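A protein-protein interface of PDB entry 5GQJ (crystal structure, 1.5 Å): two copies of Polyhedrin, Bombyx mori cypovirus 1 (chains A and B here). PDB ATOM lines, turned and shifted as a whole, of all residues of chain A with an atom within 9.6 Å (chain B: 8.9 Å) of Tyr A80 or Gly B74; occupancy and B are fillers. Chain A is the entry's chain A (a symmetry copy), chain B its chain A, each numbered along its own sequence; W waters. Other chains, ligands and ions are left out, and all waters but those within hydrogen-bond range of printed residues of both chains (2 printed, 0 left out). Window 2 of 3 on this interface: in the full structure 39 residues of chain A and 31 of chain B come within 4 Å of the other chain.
Of chain B, only Glu B73, Gly B74 and Trp B213 come within 4 Å of Tyr A80.
Of the printed residues of chain A, Gly B74 touches Ser A79 (3.5 Å) and Tyr A80 (3.7 Å).
Ser A79 touches one residue of chain B.
No residue of chain A comes within 4 Å of Gln B75.
Of the printed residues of chain A, Arg B211 touches Tyr A83 (2.7 Å).
Printed residues of chain B within 4 Å of Lys A66: Glu B73 (3.3 Å).
His A76 touches none of the printed residues of chain B.
Asp A78 touches none of the printed residues of chain B.
The nearest residue of chain B that does not touch Tyr A80 is Gln B75 (4.2 Å).
The nearest residue of chain A that does not touch Gly B74 is Tyr A83 (5.6 Å).
Hydrophobic or aromatic side chains of chain A that line the printed part of chain B: Tyr A80 and Tyr A83.
Of the 9 printed residues of chain B, 4 touch a printed residue of chain A.
Hydrophobic or aromatic side chains of chain B within 4 Å of the printed part of chain A: Trp B213.
Among the printed residues, 9 pairs touch across the chains.
Water W2 lies within hydrogen-bond range of OE1 of Glu B73 (2.6 Å), O of Ser A79 (3.0 Å) and N of Tyr A83 (3.4 Å).
Water W1 bridges OE2 of Glu B73 (2.7 Å) and ND2 of Asn A86 (3.0 Å).
O of Tyr B71 sits at hydrogen-bond distance from NE of Arg B211, at 3.4 Å.
The side-chain hydroxyl (OH) of Tyr A80 sits at hydrogen-bond distance from the side-chain carboxylate (OE2) of Glu A84.
OE1 of Gln A87 sits close to O of Tyr A83, at 3.1 Å.
OE1 of Glu A84 lies within hydrogen-bond range of N of Asp A96 (2.8 Å).
2 positions are printed for both chains.
The side-chain hydroxyl (OH) of Tyr A83 sits at hydrogen-bond distance from the backbone carbonyl oxygen (O) of Arg B211.
NE1 of Trp B213 lies within hydrogen-bond range of OH of Tyr A83 (3.2 Å).
Glu B73 touches Lys A66.
OG of Ser A79 touches CA of Gly B74 (3.5 Å).
Glu B73 touches Tyr A80 (O to CD1, 3.4 Å).
Gly B74 touches Tyr A80 (O to CB, 3.7 Å).
Tyr A80 touches Trp B213.
Glu B73 touches Tyr A83.
Glu A84 touches Trp B213.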
ATOM      1  N   LYS A  66       7.061  -5.502 -17.594  1.00  0.00           N
ATOM      2  CA  LYS A  66       8.240  -6.147 -17.051  1.00  0.00           C
ATOM      3  C   LYS A  66       9.200  -5.110 -16.528  1.00  0.00           C
ATOM      4  O   LYS A  66       9.773  -5.299 -15.422  1.00  0.00           O
ATOM      5  CB  LYS A  66       8.933  -7.001 -18.144  1.00  0.00           C
ATOM      6  CG  LYS A  66      10.164  -7.748 -17.622  1.00  0.00           C
ATOM      7  CD  LYS A  66      10.717  -8.696 -18.678  1.00  0.00           C
ATOM      8  CE  LYS A  66      11.950  -9.456 -18.221  1.00  0.00           C
ATOM      9  NZ  LYS A  66      13.186  -8.627 -18.178  1.00  0.00           N
ATOM     10  N   LYS A  69       8.733  -3.755 -13.073  1.00  0.00           N
ATOM     11  CA  LYS A  69       8.843  -4.655 -11.879  1.00  0.00           C
ATOM     12  C   LYS A  69      10.176  -4.348 -11.146  1.00  0.00           C
ATOM     13  O   LYS A  69      11.194  -3.962 -11.769  1.00  0.00           O
ATOM     14  CB  LYS A  69       8.826  -6.106 -12.284  1.00  0.00           C
ATOM     15  CG  LYS A  69       7.508  -6.541 -12.946  1.00  0.00           C
ATOM     16  CD  LYS A  69       7.696  -7.970 -13.465  1.00  0.00           C
ATOM     17  CE  LYS A  69       7.750  -8.991 -12.315  1.00  0.00           C
ATOM     18  NZ  LYS A  69       8.273 -10.255 -12.953  1.00  0.00           N
ATOM     19  N   HIS A  76      19.945 -11.509  -5.664  1.00  0.00           N
ATOM     20  CA  HIS A  76      18.963 -12.445  -6.252  1.00  0.00           C
ATOM     21  C   HIS A  76      17.613 -11.794  -6.556  1.00  0.00           C
ATOM     22  O   HIS A  76      17.133 -10.966  -5.792  1.00  0.00           O
ATOM     23  CB  HIS A  76      18.779 -13.713  -5.398  1.00  0.00           C
ATOM     24  CG  HIS A  76      19.989 -14.599  -5.391  1.00  0.00           C
ATOM     25  ND1 HIS A  76      20.423 -15.286  -6.509  1.00  0.00           N
ATOM     26  CD2 HIS A  76      20.894 -14.868  -4.416  1.00  0.00           C
ATOM     27  CE1 HIS A  76      21.515 -15.972  -6.209  1.00  0.00           C
ATOM     28  NE2 HIS A  76      21.816 -15.739  -4.941  1.00  0.00           N
ATOM     29  N   ASN A  77      17.014 -12.165  -7.698  1.00  0.00           N
ATOM     30  CA  ASN A  77      15.710 -11.614  -8.156  1.00  0.00           C
ATOM     31  C   ASN A  77      14.657 -12.674  -8.537  1.00  0.00           C
ATOM     32  O   ASN A  77      13.677 -12.357  -9.232  1.00  0.00           O
ATOM     33  CB  ASN A  77      15.917 -10.674  -9.332  1.00  0.00           C
ATOM     34  CG  ASN A  77      16.550  -9.357  -8.913  1.00  0.00           C
ATOM     35  OD1 ASN A  77      15.904  -8.501  -8.310  1.00  0.00           O
ATOM     36  ND2 ASN A  77      17.820  -9.198  -9.234  1.00  0.00           N
ATOM     37  N   ASP A  78      14.883 -13.932  -8.133  1.00  0.00           N
ATOM     38  CA  ASP A  78      13.983 -15.066  -8.481  1.00  0.00           C
ATOM     39  C   ASP A  78      13.814 -15.036 -10.034  1.00  0.00           C
ATOM     40  O   ASP A  78      12.667 -15.172 -10.520  1.00  0.00           O
ATOM     41  CB  ASP A  78      12.532 -14.943  -7.865  1.00  0.00           C
ATOM     42  CG  ASP A  78      12.357 -15.571  -6.477  1.00  0.00           C
ATOM     43  OD1 ASP A  78      13.322 -16.043  -5.908  1.00  0.00           O
ATOM     44  OD2 ASP A  78      11.205 -15.609  -5.959  1.00  0.00           O
ATOM     45  N   SER A  79      14.896 -14.760 -10.798  1.00  0.00           N
ATOM     46  CA  SER A  79      14.713 -14.433 -12.208  1.00  0.00           C
ATOM     47  C   SER A  79      13.928 -15.471 -13.023  1.00  0.00           C
ATOM     48  O   SER A  79      13.080 -15.049 -13.824  1.00  0.00           O
ATOM     49  CB  SER A  79      16.032 -13.998 -12.917  1.00  0.00           C
ATOM     50  OG  SER A  79      16.970 -15.112 -12.926  1.00  0.00           O
ATOM     51  N   TYR A  80      14.161 -16.778 -12.786  1.00  0.00           N
ATOM     52  CA  TYR A  80      13.419 -17.789 -13.549  1.00  0.00           C
ATOM     53  C   TYR A  80      11.959 -17.780 -13.110  1.00  0.00           C
ATOM     54  O   TYR A  80      11.051 -17.741 -13.950  1.00  0.00           O
ATOM     55  CB  TYR A  80      13.987 -19.252 -13.472  1.00  0.00           C
ATOM     56  CG  TYR A  80      13.157 -20.090 -14.399  1.00  0.00           C
ATOM     57  CD1 TYR A  80      13.339 -19.999 -15.809  1.00  0.00           C
ATOM     58  CD2 TYR A  80      12.113 -20.887 -13.915  1.00  0.00           C
ATOM     59  CE1 TYR A  80      12.512 -20.712 -16.695  1.00  0.00           C
ATOM     60  CE2 TYR A  80      11.249 -21.580 -14.797  1.00  0.00           C
ATOM     61  CZ  TYR A  80      11.461 -21.479 -16.181  1.00  0.00           C
ATOM     62  OH  TYR A  80      10.626 -22.183 -17.041  1.00  0.00           O
ATOM     63  N   ASP A  81      11.712 -17.818 -11.804  1.00  0.00           N
ATOM     64  CA  ASP A  81      10.290 -17.822 -11.350  1.00  0.00           C
ATOM     65  C   ASP A  81       9.557 -16.584 -11.870  1.00  0.00           C
ATOM     66  O   ASP A  81       8.352 -16.645 -12.154  1.00  0.00           O
ATOM     67  CB  ASP A  81      10.227 -17.862  -9.807  1.00  0.00           C
ATOM     68  CG  ASP A  81       8.889 -18.328  -9.303  1.00  0.00           C
ATOM     69  OD1 ASP A  81       8.388 -19.335  -9.820  1.00  0.00           O
ATOM     70  OD2 ASP A  81       8.292 -17.670  -8.411  1.00  0.00           O
ATOM     71  N   GLU A  82      10.301 -15.453 -11.951  1.00  0.00           N
ATOM     72  CA  GLU A  82       9.700 -14.216 -12.406  1.00  0.00           C
ATOM     73  C   GLU A  82       9.380 -14.167 -13.913  1.00  0.00           C
ATOM     74  O   GLU A  82       8.468 -13.474 -14.271  1.00  0.00           O
ATOM     75  CB  GLU A  82      10.503 -12.973 -11.988  1.00  0.00           C
ATOM     76  CG  GLU A  82      10.458 -12.702 -10.497  1.00  0.00           C
ATOM     77  CD  GLU A  82       9.099 -12.288  -9.941  1.00  0.00           C
ATOM     78  OE1 GLU A  82       8.306 -11.637 -10.640  1.00  0.00           O
ATOM     79  OE2 GLU A  82       8.811 -12.651  -8.755  1.00  0.00           O
ATOM     80  N   TYR A  83      10.139 -14.907 -14.742  1.00  0.00           N
ATOM     81  CA  TYR A  83       9.713 -15.165 -16.126  1.00  0.00           C
ATOM     82  C   TYR A  83       8.338 -15.860 -16.098  1.00  0.00           C
ATOM     83  O   TYR A  83       7.436 -15.474 -16.854  1.00  0.00           O
ATOM     84  CB  TYR A  83      10.788 -15.987 -16.892  1.00  0.00           C
ATOM     85  CG  TYR A  83      10.276 -16.510 -18.240  1.00  0.00           C
ATOM     86  CD1 TYR A  83      10.235 -15.686 -19.373  1.00  0.00           C
ATOM     87  CD2 TYR A  83       9.746 -17.808 -18.333  1.00  0.00           C
ATOM     88  CE1 TYR A  83       9.697 -16.155 -20.627  1.00  0.00           C
ATOM     89  CE2 TYR A  83       9.214 -18.286 -19.551  1.00  0.00           C
ATOM     90  CZ  TYR A  83       9.204 -17.479 -20.674  1.00  0.00           C
ATOM     91  OH  TYR A  83       8.660 -18.033 -21.840  1.00  0.00           O
ATOM     92  N   GLU A  84       8.181 -16.869 -15.235  1.00  0.00           N
ATOM     93  CA  GLU A  84       6.931 -17.657 -15.204  1.00  0.00           C
ATOM     94  C   GLU A  84       5.808 -16.787 -14.660  1.00  0.00           C
ATOM     95  O   GLU A  84       4.696 -16.898 -15.125  1.00  0.00           O
ATOM     96  CB  GLU A  84       7.089 -18.926 -14.315  1.00  0.00           C
ATOM     97  CG  GLU A  84       8.070 -19.908 -14.885  1.00  0.00           C
ATOM     98  CD  GLU A  84       7.472 -20.650 -16.057  1.00  0.00           C
ATOM     99  OE1 GLU A  84       6.248 -20.456 -16.273  1.00  0.00           O
ATOM    100  OE2 GLU A  84       8.239 -21.429 -16.701  1.00  0.00           O
ATOM    101  N   VAL A  85       6.109 -15.930 -13.679  1.00  0.00           N
ATOM    102  CA  VAL A  85       5.108 -14.968 -13.167  1.00  0.00           C
ATOM    103  C   VAL A  85       4.611 -14.128 -14.376  1.00  0.00           C
ATOM    104  O   VAL A  85       3.395 -13.944 -14.552  1.00  0.00           O
ATOM    105  CB  VAL A  85       5.740 -13.998 -12.139  1.00  0.00           C
ATOM    106  CG1 VAL A  85       4.889 -12.740 -11.959  1.00  0.00           C
ATOM    107  CG2 VAL A  85       5.981 -14.672 -10.780  1.00  0.00           C
ATOM    108  N   ASN A  86       5.537 -13.574 -15.188  1.00  0.00           N
ATOM    109  CA  ASN A  86       5.102 -12.753 -16.362  1.00  0.00           C
ATOM    110  C   ASN A  86       4.203 -13.553 -17.305  1.00  0.00           C
ATOM    111  O   ASN A  86       3.172 -13.008 -17.742  1.00  0.00           O
ATOM    112  CB  ASN A  86       6.317 -12.195 -17.170  1.00  0.00           C
ATOM    113  CG  ASN A  86       7.179 -11.250 -16.330  1.00  0.00           C
ATOM    114  OD1 ASN A  86       6.740 -10.788 -15.243  1.00  0.00           O
ATOM    115  ND2 ASN A  86       8.416 -11.049 -16.751  1.00  0.00           N
ATOM    116  N   GLN A  87       4.506 -14.826 -17.544  1.00  0.00           N
ATOM    117  CA  GLN A  87       3.622 -15.593 -18.414  1.00  0.00           C
ATOM    118  C   GLN A  87       2.205 -15.723 -17.868  1.00  0.00           C
ATOM    119  O   GLN A  87       1.234 -15.697 -18.630  1.00  0.00           O
ATOM    120  CB  GLN A  87       4.169 -17.010 -18.701  1.00  0.00           C
ATOM    121  CG  GLN A  87       5.638 -17.060 -19.163  1.00  0.00           C
ATOM    122  CD  GLN A  87       6.017 -15.955 -20.174  1.00  0.00           C
ATOM    123  OE1 GLN A  87       6.875 -15.087 -19.875  1.00  0.00           O
ATOM    124  NE2 GLN A  87       5.375 -15.949 -21.308  1.00  0.00           N
ATOM    125  N   SER A  88       2.071 -15.915 -16.559  1.00  0.00           N
ATOM    126  CA  SER A  88       0.741 -15.932 -15.910  1.00  0.00           C
ATOM    127  C   SER A  88       0.044 -14.618 -15.893  1.00  0.00           C
ATOM    128  O   SER A  88      -1.198 -14.592 -15.917  1.00  0.00           O
ATOM    129  CB  SER A  88       0.814 -16.414 -14.452  1.00  0.00           C
ATOM    130  OG  SER A  88       1.192 -17.774 -14.423  1.00  0.00           O
ATOM    131  N   GLY A  94      -1.185 -18.927 -17.671  1.00  0.00           N
ATOM    132  CA  GLY A  94      -0.187 -19.116 -18.746  1.00  0.00           C
ATOM    133  C   GLY A  94       1.205 -19.506 -18.280  1.00  0.00           C
ATOM    134  O   GLY A  94       2.079 -19.827 -19.116  1.00  0.00           O
ATOM    135  N   GLY A  95       1.431 -19.428 -16.968  1.00  0.00           N
ATOM    136  CA  GLY A  95       2.740 -19.690 -16.380  1.00  0.00           C
ATOM    137  C   GLY A  95       2.732 -20.816 -15.363  1.00  0.00           C
ATOM    138  O   GLY A  95       1.718 -21.439 -15.088  1.00  0.00           O
ATOM    139  N   ASP A  96       3.909 -21.113 -14.868  1.00  0.00           N
ATOM    140  CA  ASP A  96       4.145 -22.208 -13.924  1.00  0.00           C
ATOM    141  C   ASP A  96       4.957 -21.631 -12.761  1.00  0.00           C
ATOM    142  O   ASP A  96       6.053 -22.121 -12.451  1.00  0.00           O
ATOM    143  CB  ASP A  96       4.898 -23.314 -14.720  1.00  0.00           C
ATOM    144  CG  ASP A  96       5.283 -24.498 -13.890  1.00  0.00           C
ATOM    145  OD1 ASP A  96       4.465 -24.958 -13.027  1.00  0.00           O
ATOM    146  OD2 ASP A  96       6.452 -24.929 -14.115  1.00  0.00           O
ATOM    147  N   ALA A  97       4.481 -20.548 -12.138  1.00  0.00           N
ATOM    148  CA  ALA A  97       5.285 -19.899 -11.051  1.00  0.00           C
ATOM    149  C   ALA A  97       5.037 -20.488  -9.646  1.00  0.00           C
ATOM    150  O   ALA A  97       3.993 -21.122  -9.383  1.00  0.00           O
ATOM    151  CB  ALA A  97       5.075 -18.392 -11.017  1.00  0.00           C
ATOM    152  N   ARG A  98       5.968 -20.231  -8.724  1.00  0.00           N
ATOM    153  CA  ARG A  98       5.879 -20.775  -7.349  1.00  0.00           C
ATOM    154  C   ARG A  98       5.371 -19.755  -6.336  1.00  0.00           C
ATOM    155  O   ARG A  98       5.621 -19.889  -5.113  1.00  0.00           O
ATOM    156  CB  ARG A  98       7.247 -21.266  -6.904  1.00  0.00           C
ATOM    157  CG  ARG A  98       7.827 -22.340  -7.852  1.00  0.00           C
ATOM    158  CD  ARG A  98       9.220 -22.734  -7.366  1.00  0.00           C
ATOM    159  NE  ARG A  98       9.885 -23.796  -8.140  1.00  0.00           N
ATOM    160  CZ  ARG A  98      11.181 -24.119  -7.978  1.00  0.00           C
ATOM    161  NH1 ARG A  98      11.945 -23.479  -7.073  1.00  0.00           N
ATOM    162  NH2 ARG A  98      11.713 -25.087  -8.715  1.00  0.00           N
ATOM    163  N   LYS A  99       4.654 -18.728  -6.834  1.00  0.00           N
ATOM    164  CA  LYS A  99       4.050 -17.688  -5.969  1.00  0.00           C
ATOM    165  C   LYS A  99       2.765 -17.142  -6.588  1.00  0.00           C
ATOM    166  O   LYS A  99       2.630 -17.053  -7.844  1.00  0.00           O
ATOM    167  CB  LYS A  99       5.019 -16.537  -5.681  1.00  0.00           C
ATOM    168  CG  LYS A  99       5.545 -15.818  -6.926  1.00  0.00           C
ATOM    169  CD  LYS A  99       6.379 -14.637  -6.473  1.00  0.00           C
ATOM    170  CE  LYS A  99       7.752 -15.107  -6.046  1.00  0.00           C
ATOM    171  NZ  LYS A  99       8.610 -15.261  -7.289  1.00  0.00           N
ATOM    172  N   TYR B  71      17.357 -14.885 -25.883  1.00  0.00           N
ATOM    173  CA  TYR B  71      17.736 -14.705 -24.466  1.00  0.00           C
ATOM    174  C   TYR B  71      16.715 -15.488 -23.606  1.00  0.00           C
ATOM    175  O   TYR B  71      15.497 -15.218 -23.684  1.00  0.00           O
ATOM    176  CB  TYR B  71      17.762 -13.185 -24.075  1.00  0.00           C
ATOM    177  CG  TYR B  71      18.225 -13.041 -22.643  1.00  0.00           C
ATOM    178  CD1 TYR B  71      19.569 -13.336 -22.309  1.00  0.00           C
ATOM    179  CD2 TYR B  71      17.323 -12.677 -21.628  1.00  0.00           C
ATOM    180  CE1 TYR B  71      20.001 -13.285 -20.993  1.00  0.00           C
ATOM    181  CE2 TYR B  71      17.734 -12.617 -20.298  1.00  0.00           C
ATOM    182  CZ  TYR B  71      19.077 -12.923 -19.998  1.00  0.00           C
ATOM    183  OH  TYR B  71      19.553 -12.860 -18.699  1.00  0.00           O
ATOM    184  N   ARG B  72      17.201 -16.447 -22.809  1.00  0.00           N
ATOM    185  CA  ARG B  72      16.345 -17.316 -21.978  1.00  0.00           C
ATOM    186  C   ARG B  72      16.412 -16.776 -20.577  1.00  0.00           C
ATOM    187  O   ARG B  72      17.401 -16.917 -19.888  1.00  0.00           O
ATOM    188  CB  ARG B  72      16.764 -18.788 -22.066  1.00  0.00           C
ATOM    189  CG  ARG B  72      16.805 -19.288 -23.509  1.00  0.00           C
ATOM    190  CD  ARG B  72      17.076 -20.796 -23.546  1.00  0.00           C
ATOM    191  NE  ARG B  72      18.271 -21.179 -22.784  1.00  0.00           N
ATOM    192  CZ  ARG B  72      18.562 -22.434 -22.450  1.00  0.00           C
ATOM    193  NH1 ARG B  72      17.749 -23.434 -22.854  1.00  0.00           N
ATOM    194  NH2 ARG B  72      19.658 -22.703 -21.730  1.00  0.00           N
ATOM    195  N   GLU B  73      15.348 -16.116 -20.131  1.00  0.00           N
ATOM    196  CA  GLU B  73      15.362 -15.485 -18.788  1.00  0.00           C
ATOM    197  C   GLU B  73      15.468 -16.544 -17.713  1.00  0.00           C
ATOM    198  O   GLU B  73      14.740 -17.582 -17.770  1.00  0.00           O
ATOM    199  CB  GLU B  73      14.078 -14.681 -18.510  1.00  0.00           C
ATOM    200  CG  GLU B  73      13.897 -13.397 -19.321  1.00  0.00           C
ATOM    201  CD  GLU B  73      12.524 -12.788 -19.069  1.00  0.00           C
ATOM    202  OE1 GLU B  73      12.023 -12.851 -17.916  1.00  0.00           O
ATOM    203  OE2 GLU B  73      11.912 -12.273 -20.030  1.00  0.00           O
ATOM    204  N   GLY B  74      16.367 -16.296 -16.767  1.00  0.00           N
ATOM    205  CA  GLY B  74      16.600 -17.220 -15.649  1.00  0.00           C
ATOM    206  C   GLY B  74      17.265 -18.548 -15.985  1.00  0.00           C
ATOM    207  O   GLY B  74      17.254 -19.448 -15.137  1.00  0.00           O
ATOM    208  N   GLN B  75      17.796 -18.711 -17.216  1.00  0.00           N
ATOM    209  CA  GLN B  75      18.548 -19.906 -17.569  1.00  0.00           C
ATOM    210  C   GLN B  75      19.956 -19.555 -18.019  1.00  0.00           C
ATOM    211  O   GLN B  75      20.269 -18.362 -18.228  1.00  0.00           O
ATOM    212  CB  GLN B  75      17.830 -20.658 -18.697  1.00  0.00           C
ATOM    213  CG  GLN B  75      16.506 -21.281 -18.220  1.00  0.00           C
ATOM    214  CD  GLN B  75      15.764 -21.998 -19.318  1.00  0.00           C
ATOM    215  OE1 GLN B  75      14.994 -21.379 -20.061  1.00  0.00           O
ATOM    216  NE2 GLN B  75      15.992 -23.319 -19.437  1.00  0.00           N
ATOM    217  N   HIS B  76      20.810 -20.559 -18.194  1.00  0.00           N
ATOM    218  CA  HIS B  76      22.105 -20.328 -18.869  1.00  0.00           C
ATOM    219  C   HIS B  76      21.959 -19.904 -20.331  1.00  0.00           C
ATOM    220  O   HIS B  76      21.096 -20.404 -21.043  1.00  0.00           O
ATOM    221  CB  HIS B  76      23.056 -21.532 -18.741  1.00  0.00           C
ATOM    222  CG  HIS B  76      23.544 -21.750 -17.340  1.00  0.00           C
ATOM    223  ND1 HIS B  76      24.396 -20.873 -16.697  1.00  0.00           N
ATOM    224  CD2 HIS B  76      23.255 -22.717 -16.432  1.00  0.00           C
ATOM    225  CE1 HIS B  76      24.645 -21.314 -15.473  1.00  0.00           C
ATOM    226  NE2 HIS B  76      23.967 -22.437 -15.293  1.00  0.00           N
ATOM    227  N   ASN B  77      22.803 -18.957 -20.767  1.00  0.00           N
ATOM    228  CA  ASN B  77      22.783 -18.416 -22.153  1.00  0.00           C
ATOM    229  C   ASN B  77      24.148 -18.422 -22.871  1.00  0.00           C
ATOM    230  O   ASN B  77      24.328 -17.710 -23.873  1.00  0.00           O
ATOM    231  CB  ASN B  77      22.225 -17.002 -22.160  1.00  0.00           C
ATOM    232  CG  ASN B  77      20.724 -16.973 -21.916  1.00  0.00           C
ATOM    233  OD1 ASN B  77      19.929 -17.319 -22.789  1.00  0.00           O
ATOM    234  ND2 ASN B  77      20.340 -16.561 -20.724  1.00  0.00           N
ATOM    235  N   ARG B 211       9.463 -13.811 -24.856  1.00  0.00           N
ATOM    236  CA  ARG B 211       9.843 -14.993 -25.630  1.00  0.00           C
ATOM    237  C   ARG B 211       8.881 -16.100 -25.206  1.00  0.00           C
ATOM    238  O   ARG B 211       8.876 -16.490 -24.067  1.00  0.00           O
ATOM    239  CB  ARG B 211      11.273 -15.405 -25.309  1.00  0.00           C
ATOM    240  CG  ARG B 211      11.786 -16.573 -26.139  1.00  0.00           C
ATOM    241  CD  ARG B 211      13.243 -17.009 -25.858  1.00  0.00           C
ATOM    242  NE  ARG B 211      13.318 -17.633 -24.521  1.00  0.00           N
ATOM    243  CZ  ARG B 211      13.216 -18.951 -24.270  1.00  0.00           C
ATOM    244  NH1 ARG B 211      13.148 -19.852 -25.264  1.00  0.00           N
ATOM    245  NH2 ARG B 211      13.229 -19.379 -22.991  1.00  0.00           N
ATOM    246  N   TRP B 213       7.603 -20.179 -25.896  1.00  0.00           N
ATOM    247  CA  TRP B 213       8.369 -21.392 -26.089  1.00  0.00           C
ATOM    248  C   TRP B 213       8.066 -22.084 -27.379  1.00  0.00           C
ATOM    249  O   TRP B 213       8.833 -22.916 -27.774  1.00  0.00           O
ATOM    250  CB  TRP B 213       8.133 -22.403 -24.948  1.00  0.00           C
ATOM    251  CG  TRP B 213       8.723 -21.972 -23.653  1.00  0.00           C
ATOM    252  CD1 TRP B 213       9.589 -20.935 -23.439  1.00  0.00           C
ATOM    253  CD2 TRP B 213       8.580 -22.655 -22.421  1.00  0.00           C
ATOM    254  NE1 TRP B 213       9.991 -20.926 -22.094  1.00  0.00           N
ATOM    255  CE2 TRP B 213       9.371 -21.973 -21.460  1.00  0.00           C
ATOM    256  CE3 TRP B 213       7.846 -23.794 -22.024  1.00  0.00           C
ATOM    257  CZ2 TRP B 213       9.429 -22.379 -20.056  1.00  0.00           C
ATOM    258  CZ3 TRP B 213       7.880 -24.190 -20.631  1.00  0.00           C
ATOM    259  CH2 TRP B 213       8.685 -23.479 -19.684  1.00  0.00           C
HETATM  260  O   HOH W   1       9.237 -12.178 -19.404  1.00  0.00           O
HETATM  261  O   HOH W   2      12.485 -12.542 -15.420  1.00  0.00           O
